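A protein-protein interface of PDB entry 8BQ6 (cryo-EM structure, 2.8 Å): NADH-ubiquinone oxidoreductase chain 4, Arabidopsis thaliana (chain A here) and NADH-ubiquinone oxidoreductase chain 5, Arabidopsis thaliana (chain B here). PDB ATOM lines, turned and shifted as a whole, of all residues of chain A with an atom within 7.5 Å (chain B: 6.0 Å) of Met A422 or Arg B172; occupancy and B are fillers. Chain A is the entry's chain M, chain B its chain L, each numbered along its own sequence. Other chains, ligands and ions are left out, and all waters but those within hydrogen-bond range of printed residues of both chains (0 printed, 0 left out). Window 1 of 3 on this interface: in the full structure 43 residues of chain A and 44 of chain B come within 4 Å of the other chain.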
ATOM      1  N   ILE A 291      17.841  -7.158 -36.846  1.00  0.00           N
ATOM      2  CA  ILE A 291      16.826  -6.513 -36.017  1.00  0.00           C
ATOM      3  C   ILE A 291      17.341  -6.328 -34.595  1.00  0.00           C
ATOM      4  O   ILE A 291      17.291  -5.227 -34.037  1.00  0.00           O
ATOM      5  CB  ILE A 291      15.515  -7.316 -36.041  1.00  0.00           C
ATOM      6  CG1 ILE A 291      14.826  -7.153 -37.394  1.00  0.00           C
ATOM      7  CG2 ILE A 291      14.603  -6.866 -34.917  1.00  0.00           C
ATOM      8  CD1 ILE A 291      13.681  -8.098 -37.608  1.00  0.00           C
ATOM      9  N   SER A 295      19.123  -2.597 -33.601  1.00  0.00           N
ATOM     10  CA  SER A 295      18.282  -1.888 -32.641  1.00  0.00           C
ATOM     11  C   SER A 295      19.081  -1.480 -31.412  1.00  0.00           C
ATOM     12  O   SER A 295      18.848  -0.412 -30.835  1.00  0.00           O
ATOM     13  CB  SER A 295      17.088  -2.745 -32.228  1.00  0.00           C
ATOM     14  OG  SER A 295      16.117  -2.816 -33.254  1.00  0.00           O
ATOM     15  N   LEU A 318      12.890  -6.506 -40.966  1.00  0.00           N
ATOM     16  CA  LEU A 318      11.589  -7.080 -40.656  1.00  0.00           C
ATOM     17  C   LEU A 318      10.768  -7.265 -41.925  1.00  0.00           C
ATOM     18  O   LEU A 318       9.964  -8.198 -42.026  1.00  0.00           O
ATOM     19  CB  LEU A 318      10.851  -6.187 -39.667  1.00  0.00           C
ATOM     20  CG  LEU A 318       9.626  -6.806 -39.013  1.00  0.00           C
ATOM     21  CD1 LEU A 318       9.967  -8.140 -38.383  1.00  0.00           C
ATOM     22  CD2 LEU A 318       9.056  -5.846 -37.999  1.00  0.00           C
ATOM     23  N   LEU A 386       5.689   8.021 -32.421  1.00  0.00           N
ATOM     24  CA  LEU A 386       4.794   6.896 -32.157  1.00  0.00           C
ATOM     25  C   LEU A 386       4.677   5.976 -33.364  1.00  0.00           C
ATOM     26  O   LEU A 386       4.687   4.747 -33.224  1.00  0.00           O
ATOM     27  CB  LEU A 386       3.410   7.408 -31.773  1.00  0.00           C
ATOM     28  CG  LEU A 386       3.257   8.230 -30.501  1.00  0.00           C
ATOM     29  CD1 LEU A 386       1.826   8.697 -30.417  1.00  0.00           C
ATOM     30  CD2 LEU A 386       3.622   7.405 -29.290  1.00  0.00           C
ATOM     31  N   ASN A 388       6.866   5.485 -35.541  1.00  0.00           N
ATOM     32  CA  ASN A 388       8.096   4.719 -35.650  1.00  0.00           C
ATOM     33  C   ASN A 388       8.151   3.567 -34.655  1.00  0.00           C
ATOM     34  O   ASN A 388       8.877   2.597 -34.891  1.00  0.00           O
ATOM     35  CB  ASN A 388       9.299   5.637 -35.469  1.00  0.00           C
ATOM     36  CG  ASN A 388      10.529   5.098 -36.141  1.00  0.00           C
ATOM     37  OD1 ASN A 388      10.601   5.033 -37.364  1.00  0.00           O
ATOM     38  ND2 ASN A 388      11.512   4.712 -35.345  1.00  0.00           N
ATOM     39  N   MET A 389       7.400   3.651 -33.559  1.00  0.00           N
ATOM     40  CA  MET A 389       7.271   2.568 -32.592  1.00  0.00           C
ATOM     41  C   MET A 389       6.208   1.551 -32.978  1.00  0.00           C
ATOM     42  O   MET A 389       5.905   0.665 -32.172  1.00  0.00           O
ATOM     43  CB  MET A 389       6.935   3.125 -31.205  1.00  0.00           C
ATOM     44  CG  MET A 389       7.667   4.388 -30.847  1.00  0.00           C
ATOM     45  SD  MET A 389       7.397   4.941 -29.156  1.00  0.00           S
ATOM     46  CE  MET A 389       6.869   3.425 -28.368  1.00  0.00           C
ATOM     47  N   SER A 390       5.630   1.662 -34.175  1.00  0.00           N
ATOM     48  CA  SER A 390       4.556   0.776 -34.625  1.00  0.00           C
ATOM     49  C   SER A 390       3.382   0.771 -33.651  1.00  0.00           C
ATOM     50  O   SER A 390       2.861  -0.288 -33.297  1.00  0.00           O
ATOM     51  CB  SER A 390       5.064  -0.650 -34.850  1.00  0.00           C
ATOM     52  OG  SER A 390       5.708  -0.768 -36.105  1.00  0.00           O
ATOM     53  N   LEU A 391       2.975   1.948 -33.199  1.00  0.00           N
ATOM     54  CA  LEU A 391       1.817   2.056 -32.328  1.00  0.00           C
ATOM     55  C   LEU A 391       0.555   1.665 -33.092  1.00  0.00           C
ATOM     56  O   LEU A 391       0.370   2.104 -34.237  1.00  0.00           O
ATOM     57  CB  LEU A 391       1.690   3.486 -31.807  1.00  0.00           C
ATOM     58  CG  LEU A 391       0.705   3.718 -30.664  1.00  0.00           C
ATOM     59  CD1 LEU A 391       1.372   3.462 -29.325  1.00  0.00           C
ATOM     60  CD2 LEU A 391       0.128   5.119 -30.739  1.00  0.00           C
ATOM     61  N   PRO A 392      -0.319   0.835 -32.517  1.00  0.00           N
ATOM     62  CA  PRO A 392      -1.581   0.517 -33.194  1.00  0.00           C
ATOM     63  C   PRO A 392      -2.387   1.772 -33.479  1.00  0.00           C
ATOM     64  O   PRO A 392      -2.494   2.672 -32.643  1.00  0.00           O
ATOM     65  CB  PRO A 392      -2.296  -0.399 -32.198  1.00  0.00           C
ATOM     66  CG  PRO A 392      -1.201  -1.042 -31.456  1.00  0.00           C
ATOM     67  CD  PRO A 392      -0.107  -0.014 -31.334  1.00  0.00           C
ATOM     68  N   PHE A 397       2.004  -0.080 -37.806  1.00  0.00           N
ATOM     69  CA  PHE A 397       1.556  -1.229 -37.029  1.00  0.00           C
ATOM     70  C   PHE A 397       0.901  -2.277 -37.922  1.00  0.00           C
ATOM     71  O   PHE A 397       1.016  -3.481 -37.661  1.00  0.00           O
ATOM     72  CB  PHE A 397       0.600  -0.789 -35.925  1.00  0.00           C
ATOM     73  CG  PHE A 397      -0.130  -1.927 -35.288  1.00  0.00           C
ATOM     74  CD1 PHE A 397       0.505  -2.748 -34.377  1.00  0.00           C
ATOM     75  CD2 PHE A 397      -1.441  -2.196 -35.626  1.00  0.00           C
ATOM     76  CE1 PHE A 397      -0.162  -3.805 -33.806  1.00  0.00           C
ATOM     77  CE2 PHE A 397      -2.108  -3.249 -35.060  1.00  0.00           C
ATOM     78  CZ  PHE A 397      -1.470  -4.054 -34.149  1.00  0.00           C
ATOM     79  N   GLU A 400       3.633  -4.257 -39.642  1.00  0.00           N
ATOM     80  CA  GLU A 400       4.432  -4.968 -38.650  1.00  0.00           C
ATOM     81  C   GLU A 400       3.721  -6.216 -38.149  1.00  0.00           C
ATOM     82  O   GLU A 400       4.311  -7.300 -38.091  1.00  0.00           O
ATOM     83  CB  GLU A 400       4.761  -4.039 -37.486  1.00  0.00           C
ATOM     84  CG  GLU A 400       5.913  -4.523 -36.632  1.00  0.00           C
ATOM     85  CD  GLU A 400       5.512  -4.789 -35.196  1.00  0.00           C
ATOM     86  OE1 GLU A 400       4.330  -4.587 -34.851  1.00  0.00           O
ATOM     87  OE2 GLU A 400       6.379  -5.202 -34.403  1.00  0.00           O
ATOM     88  N   PHE A 401       2.451  -6.078 -37.766  1.00  0.00           N
ATOM     89  CA  PHE A 401       1.725  -7.206 -37.196  1.00  0.00           C
ATOM     90  C   PHE A 401       1.440  -8.274 -38.240  1.00  0.00           C
ATOM     91  O   PHE A 401       1.486  -9.473 -37.941  1.00  0.00           O
ATOM     92  CB  PHE A 401       0.422  -6.731 -36.565  1.00  0.00           C
ATOM     93  CG  PHE A 401      -0.099  -7.656 -35.523  1.00  0.00           C
ATOM     94  CD1 PHE A 401       0.373  -7.595 -34.228  1.00  0.00           C
ATOM     95  CD2 PHE A 401      -1.046  -8.611 -35.842  1.00  0.00           C
ATOM     96  CE1 PHE A 401      -0.103  -8.458 -33.271  1.00  0.00           C
ATOM     97  CE2 PHE A 401      -1.524  -9.474 -34.887  1.00  0.00           C
ATOM     98  CZ  PHE A 401      -1.053  -9.399 -33.603  1.00  0.00           C
ATOM     99  N   LEU A 404       4.474 -10.382 -38.649  1.00  0.00           N
ATOM    100  CA  LEU A 404       4.601 -11.294 -37.519  1.00  0.00           C
ATOM    101  C   LEU A 404       3.585 -12.429 -37.604  1.00  0.00           C
ATOM    102  O   LEU A 404       3.889 -13.569 -37.236  1.00  0.00           O
ATOM    103  CB  LEU A 404       4.446 -10.517 -36.215  1.00  0.00           C
ATOM    104  CG  LEU A 404       5.543  -9.491 -35.930  1.00  0.00           C
ATOM    105  CD1 LEU A 404       5.188  -8.668 -34.709  1.00  0.00           C
ATOM    106  CD2 LEU A 404       6.890 -10.169 -35.748  1.00  0.00           C
ATOM    107  N   ALA A 415       9.567 -15.476 -35.679  1.00  0.00           N
ATOM    108  CA  ALA A 415       8.539 -14.511 -35.304  1.00  0.00           C
ATOM    109  C   ALA A 415       8.750 -14.004 -33.882  1.00  0.00           C
ATOM    110  O   ALA A 415       8.369 -12.875 -33.554  1.00  0.00           O
ATOM    111  CB  ALA A 415       7.152 -15.134 -35.445  1.00  0.00           C
ATOM    112  N   LEU A 417      11.842 -13.733 -32.285  1.00  0.00           N
ATOM    113  CA  LEU A 417      12.979 -12.823 -32.321  1.00  0.00           C
ATOM    114  C   LEU A 417      12.611 -11.517 -33.011  1.00  0.00           C
ATOM    115  O   LEU A 417      13.054 -10.441 -32.594  1.00  0.00           O
ATOM    116  CB  LEU A 417      14.157 -13.500 -33.017  1.00  0.00           C
ATOM    117  CG  LEU A 417      14.653 -14.769 -32.325  1.00  0.00           C
ATOM    118  CD1 LEU A 417      15.638 -15.508 -33.203  1.00  0.00           C
ATOM    119  CD2 LEU A 417      15.290 -14.422 -30.992  1.00  0.00           C
ATOM    120  N   ALA A 418      11.798 -11.592 -34.065  1.00  0.00           N
ATOM    121  CA  ALA A 418      11.360 -10.385 -34.754  1.00  0.00           C
ATOM    122  C   ALA A 418      10.434  -9.542 -33.887  1.00  0.00           C
ATOM    123  O   ALA A 418      10.430  -8.311 -34.004  1.00  0.00           O
ATOM    124  CB  ALA A 418      10.673 -10.755 -36.066  1.00  0.00           C
ATOM    125  N   ALA A 419       9.645 -10.173 -33.017  1.00  0.00           N
ATOM    126  CA  ALA A 419       8.780  -9.413 -32.125  1.00  0.00           C
ATOM    127  C   ALA A 419       9.559  -8.693 -31.032  1.00  0.00           C
ATOM    128  O   ALA A 419       8.978  -7.872 -30.316  1.00  0.00           O
ATOM    129  CB  ALA A 419       7.727 -10.327 -31.498  1.00  0.00           C
ATOM    130  N   LEU A 420      10.855  -8.980 -30.880  1.00  0.00           N
ATOM    131  CA  LEU A 420      11.649  -8.269 -29.884  1.00  0.00           C
ATOM    132  C   LEU A 420      11.865  -6.814 -30.267  1.00  0.00           C
ATOM    133  O   LEU A 420      12.203  -5.990 -29.411  1.00  0.00           O
ATOM    134  CB  LEU A 420      12.996  -8.958 -29.683  1.00  0.00           C
ATOM    135  CG  LEU A 420      12.959 -10.241 -28.862  1.00  0.00           C
ATOM    136  CD1 LEU A 420      14.201 -11.070 -29.124  1.00  0.00           C
ATOM    137  CD2 LEU A 420      12.824  -9.910 -27.391  1.00  0.00           C
ATOM    138  N   GLY A 421      11.676  -6.481 -31.545  1.00  0.00           N
ATOM    139  CA  GLY A 421      11.818  -5.099 -31.968  1.00  0.00           C
ATOM    140  C   GLY A 421      10.732  -4.199 -31.415  1.00  0.00           C
ATOM    141  O   GLY A 421      10.877  -2.975 -31.398  1.00  0.00           O
ATOM    142  N   MET A 422       9.621  -4.789 -30.964  1.00  0.00           N
ATOM    143  CA  MET A 422       8.601  -4.001 -30.278  1.00  0.00           C
ATOM    144  C   MET A 422       9.157  -3.389 -29.001  1.00  0.00           C
ATOM    145  O   MET A 422       8.843  -2.243 -28.663  1.00  0.00           O
ATOM    146  CB  MET A 422       7.376  -4.862 -29.961  1.00  0.00           C
ATOM    147  CG  MET A 422       6.688  -5.454 -31.180  1.00  0.00           C
ATOM    148  SD  MET A 422       5.499  -6.755 -30.780  1.00  0.00           S
ATOM    149  CE  MET A 422       4.669  -6.058 -29.352  1.00  0.00           C
ATOM    150  N   ILE A 423       9.973  -4.147 -28.269  1.00  0.00           N
ATOM    151  CA  ILE A 423      10.570  -3.612 -27.052  1.00  0.00           C
ATOM    152  C   ILE A 423      11.726  -2.680 -27.385  1.00  0.00           C
ATOM    153  O   ILE A 423      11.816  -1.570 -26.849  1.00  0.00           O
ATOM    154  CB  ILE A 423      11.015  -4.756 -26.123  1.00  0.00           C
ATOM    155  CG1 ILE A 423       9.833  -5.660 -25.768  1.00  0.00           C
ATOM    156  CG2 ILE A 423      11.649  -4.202 -24.863  1.00  0.00           C
ATOM    157  CD1 ILE A 423      10.246  -7.043 -25.326  1.00  0.00           C
ATOM    158  N   LEU A 424      12.618  -3.108 -28.281  1.00  0.00           N
ATOM    159  CA  LEU A 424      13.798  -2.310 -28.597  1.00  0.00           C
ATOM    160  C   LEU A 424      13.433  -1.032 -29.341  1.00  0.00           C
ATOM    161  O   LEU A 424      13.952   0.044 -29.025  1.00  0.00           O
ATOM    162  CB  LEU A 424      14.786  -3.147 -29.407  1.00  0.00           C
ATOM    163  CG  LEU A 424      15.438  -4.298 -28.641  1.00  0.00           C
ATOM    164  CD1 LEU A 424      16.392  -5.081 -29.525  1.00  0.00           C
ATOM    165  CD2 LEU A 424      16.168  -3.746 -27.438  1.00  0.00           C
ATOM    166  N   GLY A 425      12.536  -1.128 -30.325  1.00  0.00           N
ATOM    167  CA  GLY A 425      12.162   0.050 -31.091  1.00  0.00           C
ATOM    168  C   GLY A 425      11.460   1.098 -30.250  1.00  0.00           C
ATOM    169  O   GLY A 425      11.543   2.295 -30.533  1.00  0.00           O
ATOM    170  N   ALA A 426      10.745   0.659 -29.214  1.00  0.00           N
ATOM    171  CA  ALA A 426      10.128   1.600 -28.287  1.00  0.00           C
ATOM    172  C   ALA A 426      11.186   2.327 -27.470  1.00  0.00           C
ATOM    173  O   ALA A 426      11.042   3.515 -27.157  1.00  0.00           O
ATOM    174  CB  ALA A 426       9.154   0.864 -27.369  1.00  0.00           C
ATOM    175  N   ALA A 427      12.258   1.621 -27.112  1.00  0.00           N
ATOM    176  CA  ALA A 427      13.252   2.177 -26.204  1.00  0.00           C
ATOM    177  C   ALA A 427      14.012   3.334 -26.838  1.00  0.00           C
ATOM    178  O   ALA A 427      14.245   4.362 -26.195  1.00  0.00           O
ATOM    179  CB  ALA A 427      14.214   1.079 -25.753  1.00  0.00           C
ATOM    180  N   SER A 429      13.113   5.118 -29.603  1.00  0.00           N
ATOM    181  CA  SER A 429      12.264   6.191 -30.118  1.00  0.00           C
ATOM    182  C   SER A 429      11.843   7.144 -29.009  1.00  0.00           C
ATOM    183  O   SER A 429      11.822   8.365 -29.198  1.00  0.00           O
ATOM    184  CB  SER A 429      11.031   5.621 -30.821  1.00  0.00           C
ATOM    185  OG  SER A 429      11.361   4.537 -31.663  1.00  0.00           O
ATOM    186  N   LEU A 430      11.482   6.605 -27.845  1.00  0.00           N
ATOM    187  CA  LEU A 430      11.052   7.470 -26.753  1.00  0.00           C
ATOM    188  C   LEU A 430      12.236   8.156 -26.091  1.00  0.00           C
ATOM    189  O   LEU A 430      12.126   9.303 -25.646  1.00  0.00           O
ATOM    190  CB  LEU A 430      10.261   6.672 -25.726  1.00  0.00           C
ATOM    191  CG  LEU A 430       8.817   6.363 -26.098  1.00  0.00           C
ATOM    192  CD1 LEU A 430       8.178   5.714 -24.916  1.00  0.00           C
ATOM    193  CD2 LEU A 430       8.056   7.619 -26.500  1.00  0.00           C
ATOM    194  N   PHE B 137      -5.979  -4.981 -28.414  1.00  0.00           N
ATOM    195  CA  PHE B 137      -4.575  -4.595 -28.456  1.00  0.00           C
ATOM    196  C   PHE B 137      -4.430  -3.096 -28.687  1.00  0.00           C
ATOM    197  O   PHE B 137      -3.539  -2.456 -28.118  1.00  0.00           O
ATOM    198  CB  PHE B 137      -3.858  -5.400 -29.537  1.00  0.00           C
ATOM    199  CG  PHE B 137      -2.366  -5.378 -29.421  1.00  0.00           C
ATOM    200  CD1 PHE B 137      -1.718  -6.179 -28.499  1.00  0.00           C
ATOM    201  CD2 PHE B 137      -1.608  -4.582 -30.255  1.00  0.00           C
ATOM    202  CE1 PHE B 137      -0.340  -6.164 -28.399  1.00  0.00           C
ATOM    203  CE2 PHE B 137      -0.231  -4.567 -30.160  1.00  0.00           C
ATOM    204  CZ  PHE B 137       0.402  -5.356 -29.233  1.00  0.00           C
ATOM    205  N   GLU B 141      -2.477  -0.783 -26.026  1.00  0.00           N
ATOM    206  CA  GLU B 141      -1.359   0.115 -26.297  1.00  0.00           C
ATOM    207  C   GLU B 141      -1.732   1.565 -26.030  1.00  0.00           C
ATOM    208  O   GLU B 141      -0.907   2.343 -25.538  1.00  0.00           O
ATOM    209  CB  GLU B 141      -0.884  -0.059 -27.737  1.00  0.00           C
ATOM    210  CG  GLU B 141      -0.204  -1.379 -27.996  1.00  0.00           C
ATOM    211  CD  GLU B 141       1.299  -1.287 -27.861  1.00  0.00           C
ATOM    212  OE1 GLU B 141       1.938  -0.603 -28.686  1.00  0.00           O
ATOM    213  OE2 GLU B 141       1.845  -1.906 -26.929  1.00  0.00           O
ATOM    214  N   ALA B 167       7.727   2.877 -17.224  1.00  0.00           N
ATOM    215  CA  ALA B 167       6.370   2.353 -17.327  1.00  0.00           C
ATOM    216  C   ALA B 167       6.099   1.809 -18.724  1.00  0.00           C
ATOM    217  O   ALA B 167       5.523   0.727 -18.881  1.00  0.00           O
ATOM    218  CB  ALA B 167       5.359   3.440 -16.966  1.00  0.00           C
ATOM    219  N   MET B 168       6.530   2.540 -19.753  1.00  0.00           N
ATOM    220  CA  MET B 168       6.245   2.136 -21.125  1.00  0.00           C
ATOM    221  C   MET B 168       7.115   0.962 -21.566  1.00  0.00           C
ATOM    222  O   MET B 168       6.669   0.098 -22.328  1.00  0.00           O
ATOM    223  CB  MET B 168       6.431   3.323 -22.068  1.00  0.00           C
ATOM    224  CG  MET B 168       6.701   2.907 -23.494  1.00  0.00           C
ATOM    225  SD  MET B 168       5.217   2.961 -24.505  1.00  0.00           S
ATOM    226  CE  MET B 168       4.804   4.695 -24.384  1.00  0.00           C
ATOM    227  N   LEU B 169       8.367   0.919 -21.107  1.00  0.00           N
ATOM    228  CA  LEU B 169       9.240  -0.185 -21.493  1.00  0.00           C
ATOM    229  C   LEU B 169       8.816  -1.491 -20.836  1.00  0.00           C
ATOM    230  O   LEU B 169       8.832  -2.547 -21.478  1.00  0.00           O
ATOM    231  CB  LEU B 169      10.693   0.136 -21.154  1.00  0.00           C
ATOM    232  CG  LEU B 169      11.308   1.188 -22.069  1.00  0.00           C
ATOM    233  CD1 LEU B 169      12.720   1.530 -21.638  1.00  0.00           C
ATOM    234  CD2 LEU B 169      11.279   0.685 -23.493  1.00  0.00           C
ATOM    235  N   VAL B 170       8.447  -1.444 -19.554  1.00  0.00           N
ATOM    236  CA  VAL B 170       7.986  -2.651 -18.870  1.00  0.00           C
ATOM    237  C   VAL B 170       6.710  -3.174 -19.510  1.00  0.00           C
ATOM    238  O   VAL B 170       6.513  -4.389 -19.640  1.00  0.00           O
ATOM    239  CB  VAL B 170       7.799  -2.380 -17.366  1.00  0.00           C
ATOM    240  CG1 VAL B 170       7.046  -3.516 -16.719  1.00  0.00           C
ATOM    241  CG2 VAL B 170       9.143  -2.237 -16.695  1.00  0.00           C
ATOM    242  N   ASN B 171       5.820  -2.274 -19.922  1.00  0.00           N
ATOM    243  CA  ASN B 171       4.562  -2.721 -20.505  1.00  0.00           C
ATOM    244  C   ASN B 171       4.758  -3.234 -21.924  1.00  0.00           C
ATOM    245  O   ASN B 171       4.025  -4.119 -22.376  1.00  0.00           O
ATOM    246  CB  ASN B 171       3.540  -1.592 -20.463  1.00  0.00           C
ATOM    247  CG  ASN B 171       2.933  -1.430 -19.093  1.00  0.00           C
ATOM    248  OD1 ASN B 171       2.081  -2.216 -18.682  1.00  0.00           O
ATOM    249  ND2 ASN B 171       3.376  -0.412 -18.368  1.00  0.00           N
ATOM    250  N   ARG B 172       5.752  -2.702 -22.642  1.00  0.00           N
ATOM    251  CA  ARG B 172       6.045  -3.231 -23.969  1.00  0.00           C
ATOM    252  C   ARG B 172       6.522  -4.678 -23.881  1.00  0.00           C
ATOM    253  O   ARG B 172       6.261  -5.480 -24.785  1.00  0.00           O
ATOM    254  CB  ARG B 172       7.074  -2.351 -24.682  1.00  0.00           C
ATOM    255  CG  ARG B 172       6.461  -1.326 -25.646  1.00  0.00           C
ATOM    256  CD  ARG B 172       5.982  -1.984 -26.936  1.00  0.00           C
ATOM    257  NE  ARG B 172       5.248  -1.075 -27.810  1.00  0.00           N
ATOM    258  CZ  ARG B 172       5.717  -0.568 -28.943  1.00  0.00           C
ATOM    259  NH1 ARG B 172       6.940  -0.836 -29.368  1.00  0.00           N
ATOM    260  NH2 ARG B 172       4.933   0.221 -29.674  1.00  0.00           N
ATOM    261  N   VAL B 173       7.208  -5.038 -22.793  1.00  0.00           N
ATOM    262  CA  VAL B 173       7.533  -6.443 -22.569  1.00  0.00           C
ATOM    263  C   VAL B 173       6.254  -7.255 -22.403  1.00  0.00           C
ATOM    264  O   VAL B 173       6.120  -8.353 -22.957  1.00  0.00           O
ATOM    265  CB  VAL B 173       8.468  -6.602 -21.356  1.00  0.00           C
ATOM    266  CG1 VAL B 173       8.604  -8.072 -20.982  1.00  0.00           C
ATOM    267  CG2 VAL B 173       9.832  -6.004 -21.649  1.00  0.00           C
ATOM    268  N   GLY B 174       5.293  -6.727 -21.643  1.00  0.00           N
ATOM    269  CA  GLY B 174       3.997  -7.379 -21.547  1.00  0.00           C
ATOM    270  C   GLY B 174       3.259  -7.421 -22.871  1.00  0.00           C
ATOM    271  O   GLY B 174       2.602  -8.415 -23.192  1.00  0.00           O
ATOM    272  N   ASP B 175       3.341  -6.339 -23.653  1.00  0.00           N
ATOM    273  CA  ASP B 175       2.736  -6.339 -24.983  1.00  0.00           C
ATOM    274  C   ASP B 175       3.431  -7.329 -25.905  1.00  0.00           C
ATOM    275  O   ASP B 175       2.802  -7.900 -26.802  1.00  0.00           O
ATOM    276  CB  ASP B 175       2.785  -4.940 -25.593  1.00  0.00           C
ATOM    277  CG  ASP B 175       1.804  -3.987 -24.955  1.00  0.00           C
ATOM    278  OD1 ASP B 175       2.234  -3.134 -24.154  1.00  0.00           O
ATOM    279  OD2 ASP B 175       0.604  -4.067 -25.278  1.00  0.00           O
ATOM    280  N   PHE B 176       4.738  -7.518 -25.720  1.00  0.00           N
ATOM    281  CA  PHE B 176       5.465  -8.508 -26.506  1.00  0.00           C
ATOM    282  C   PHE B 176       4.860  -9.894 -26.321  1.00  0.00           C
ATOM    283  O   PHE B 176       4.548 -10.585 -27.296  1.00  0.00           O
ATOM    284  CB  PHE B 176       6.941  -8.482 -26.104  1.00  0.00           C
ATOM    285  CG  PHE B 176       7.701  -9.721 -26.467  1.00  0.00           C
ATOM    286  CD1 PHE B 176       8.066  -9.972 -27.775  1.00  0.00           C
ATOM    287  CD2 PHE B 176       8.068 -10.627 -25.489  1.00  0.00           C
ATOM    288  CE1 PHE B 176       8.773 -11.108 -28.103  1.00  0.00           C
ATOM    289  CE2 PHE B 176       8.772 -11.766 -25.813  1.00  0.00           C
ATOM    290  CZ  PHE B 176       9.126 -12.006 -27.121  1.00  0.00           C
ATOM    291  N   GLY B 177       4.658 -10.304 -25.067  1.00  0.00           N
ATOM    292  CA  GLY B 177       4.021 -11.585 -24.814  1.00  0.00           C
ATOM    293  C   GLY B 177       2.570 -11.617 -25.250  1.00  0.00           C
ATOM    294  O   GLY B 177       2.105 -12.608 -25.817  1.00  0.00           O
ATOM    295  N   ALA B 179       1.116  -9.947 -27.670  1.00  0.00           N
ATOM    296  CA  ALA B 179       1.048 -10.052 -29.123  1.00  0.00           C
ATOM    297  C   ALA B 179       1.348 -11.470 -29.590  1.00  0.00           C
ATOM    298  O   ALA B 179       0.710 -11.970 -30.522  1.00  0.00           O
ATOM    299  CB  ALA B 179       2.012  -9.057 -29.766  1.00  0.00           C
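Hydrophobic or aromatic side chains of chain A within 4 Å of the printed part of chain B: Met A389, Pro A392, Phe A397, Ala A419, Met A422, Ile A423, Ala A426, Ala A427 and Leu A430. Printed residues of chain B that touch a printed residue of chain A: Phe B137, Glu B141, Met B168, Leu B169, Arg B172, Val B173, Asp B175 and Phe B176. Hydrophobic or aromatic side chains of chain B within 4 Å of the printed part of chain A: Phe B137, Met B168, Leu B169, Val B173 and Phe B176. Among the printed residues, no Asp or Glu carboxylate lies within 4 Å of a Lys or Arg side-chain nitrogen of the other chain.
Of chain B, only Arg B172, Asp B175 and Phe B176 come within 4 Å of Met A422. Of chain A, only Met A389, Met A422, Ile A423 and Ala A426 come within 4 Å of Arg B172. Printed residues of chain A within 4 Å of Phe B137: Pro A392 (3.8 Å) and Phe A397 (3.7 Å). Of the printed residues of chain B, Ala A419 touches Phe B176 (3.4 Å). Of the printed residues of chain B, Leu A430 touches Met B168 (3.5 Å). Of the printed residues of chain B, Ala A426 touches Arg B172. Leu A420 touches none of the printed residues of chain B. Ile A291 touches none of the printed residues of chain B. The nearest residue of chain B that does not touch Met A422 is Ala B179 (4.03 Å).
Among the printed residues, pairs that only touch across the chains: Pro A392 with Glu B141, Ala A419 with Phe B176, Ala A426 with Arg B172, Leu A430 with Met B168, Met A422 with Asp B175, Ala A427 with Leu B169, Ile A423 with Phe B176, Ile A423 with Arg B172, Phe A397 with Phe B137, Pro A392 with Phe B137, Met A422 with Phe B176 and Ile A423 with Val B173.
OE1 of Glu B141 is in salt-bridge range of NH2 of Arg B172 (3.3 Å). OD1 of Asp B175 lies close to O of Asn B171, 2.7 Å away.
O of Met A389 lies within hydrogen-bond range of NH2 of Arg B172 (2.7 Å). The guanidinium group (NH1) of Arg B172 is in hydrogen-bond range of the backbone carbonyl oxygen (O) of Met A422 (2.5 Å).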
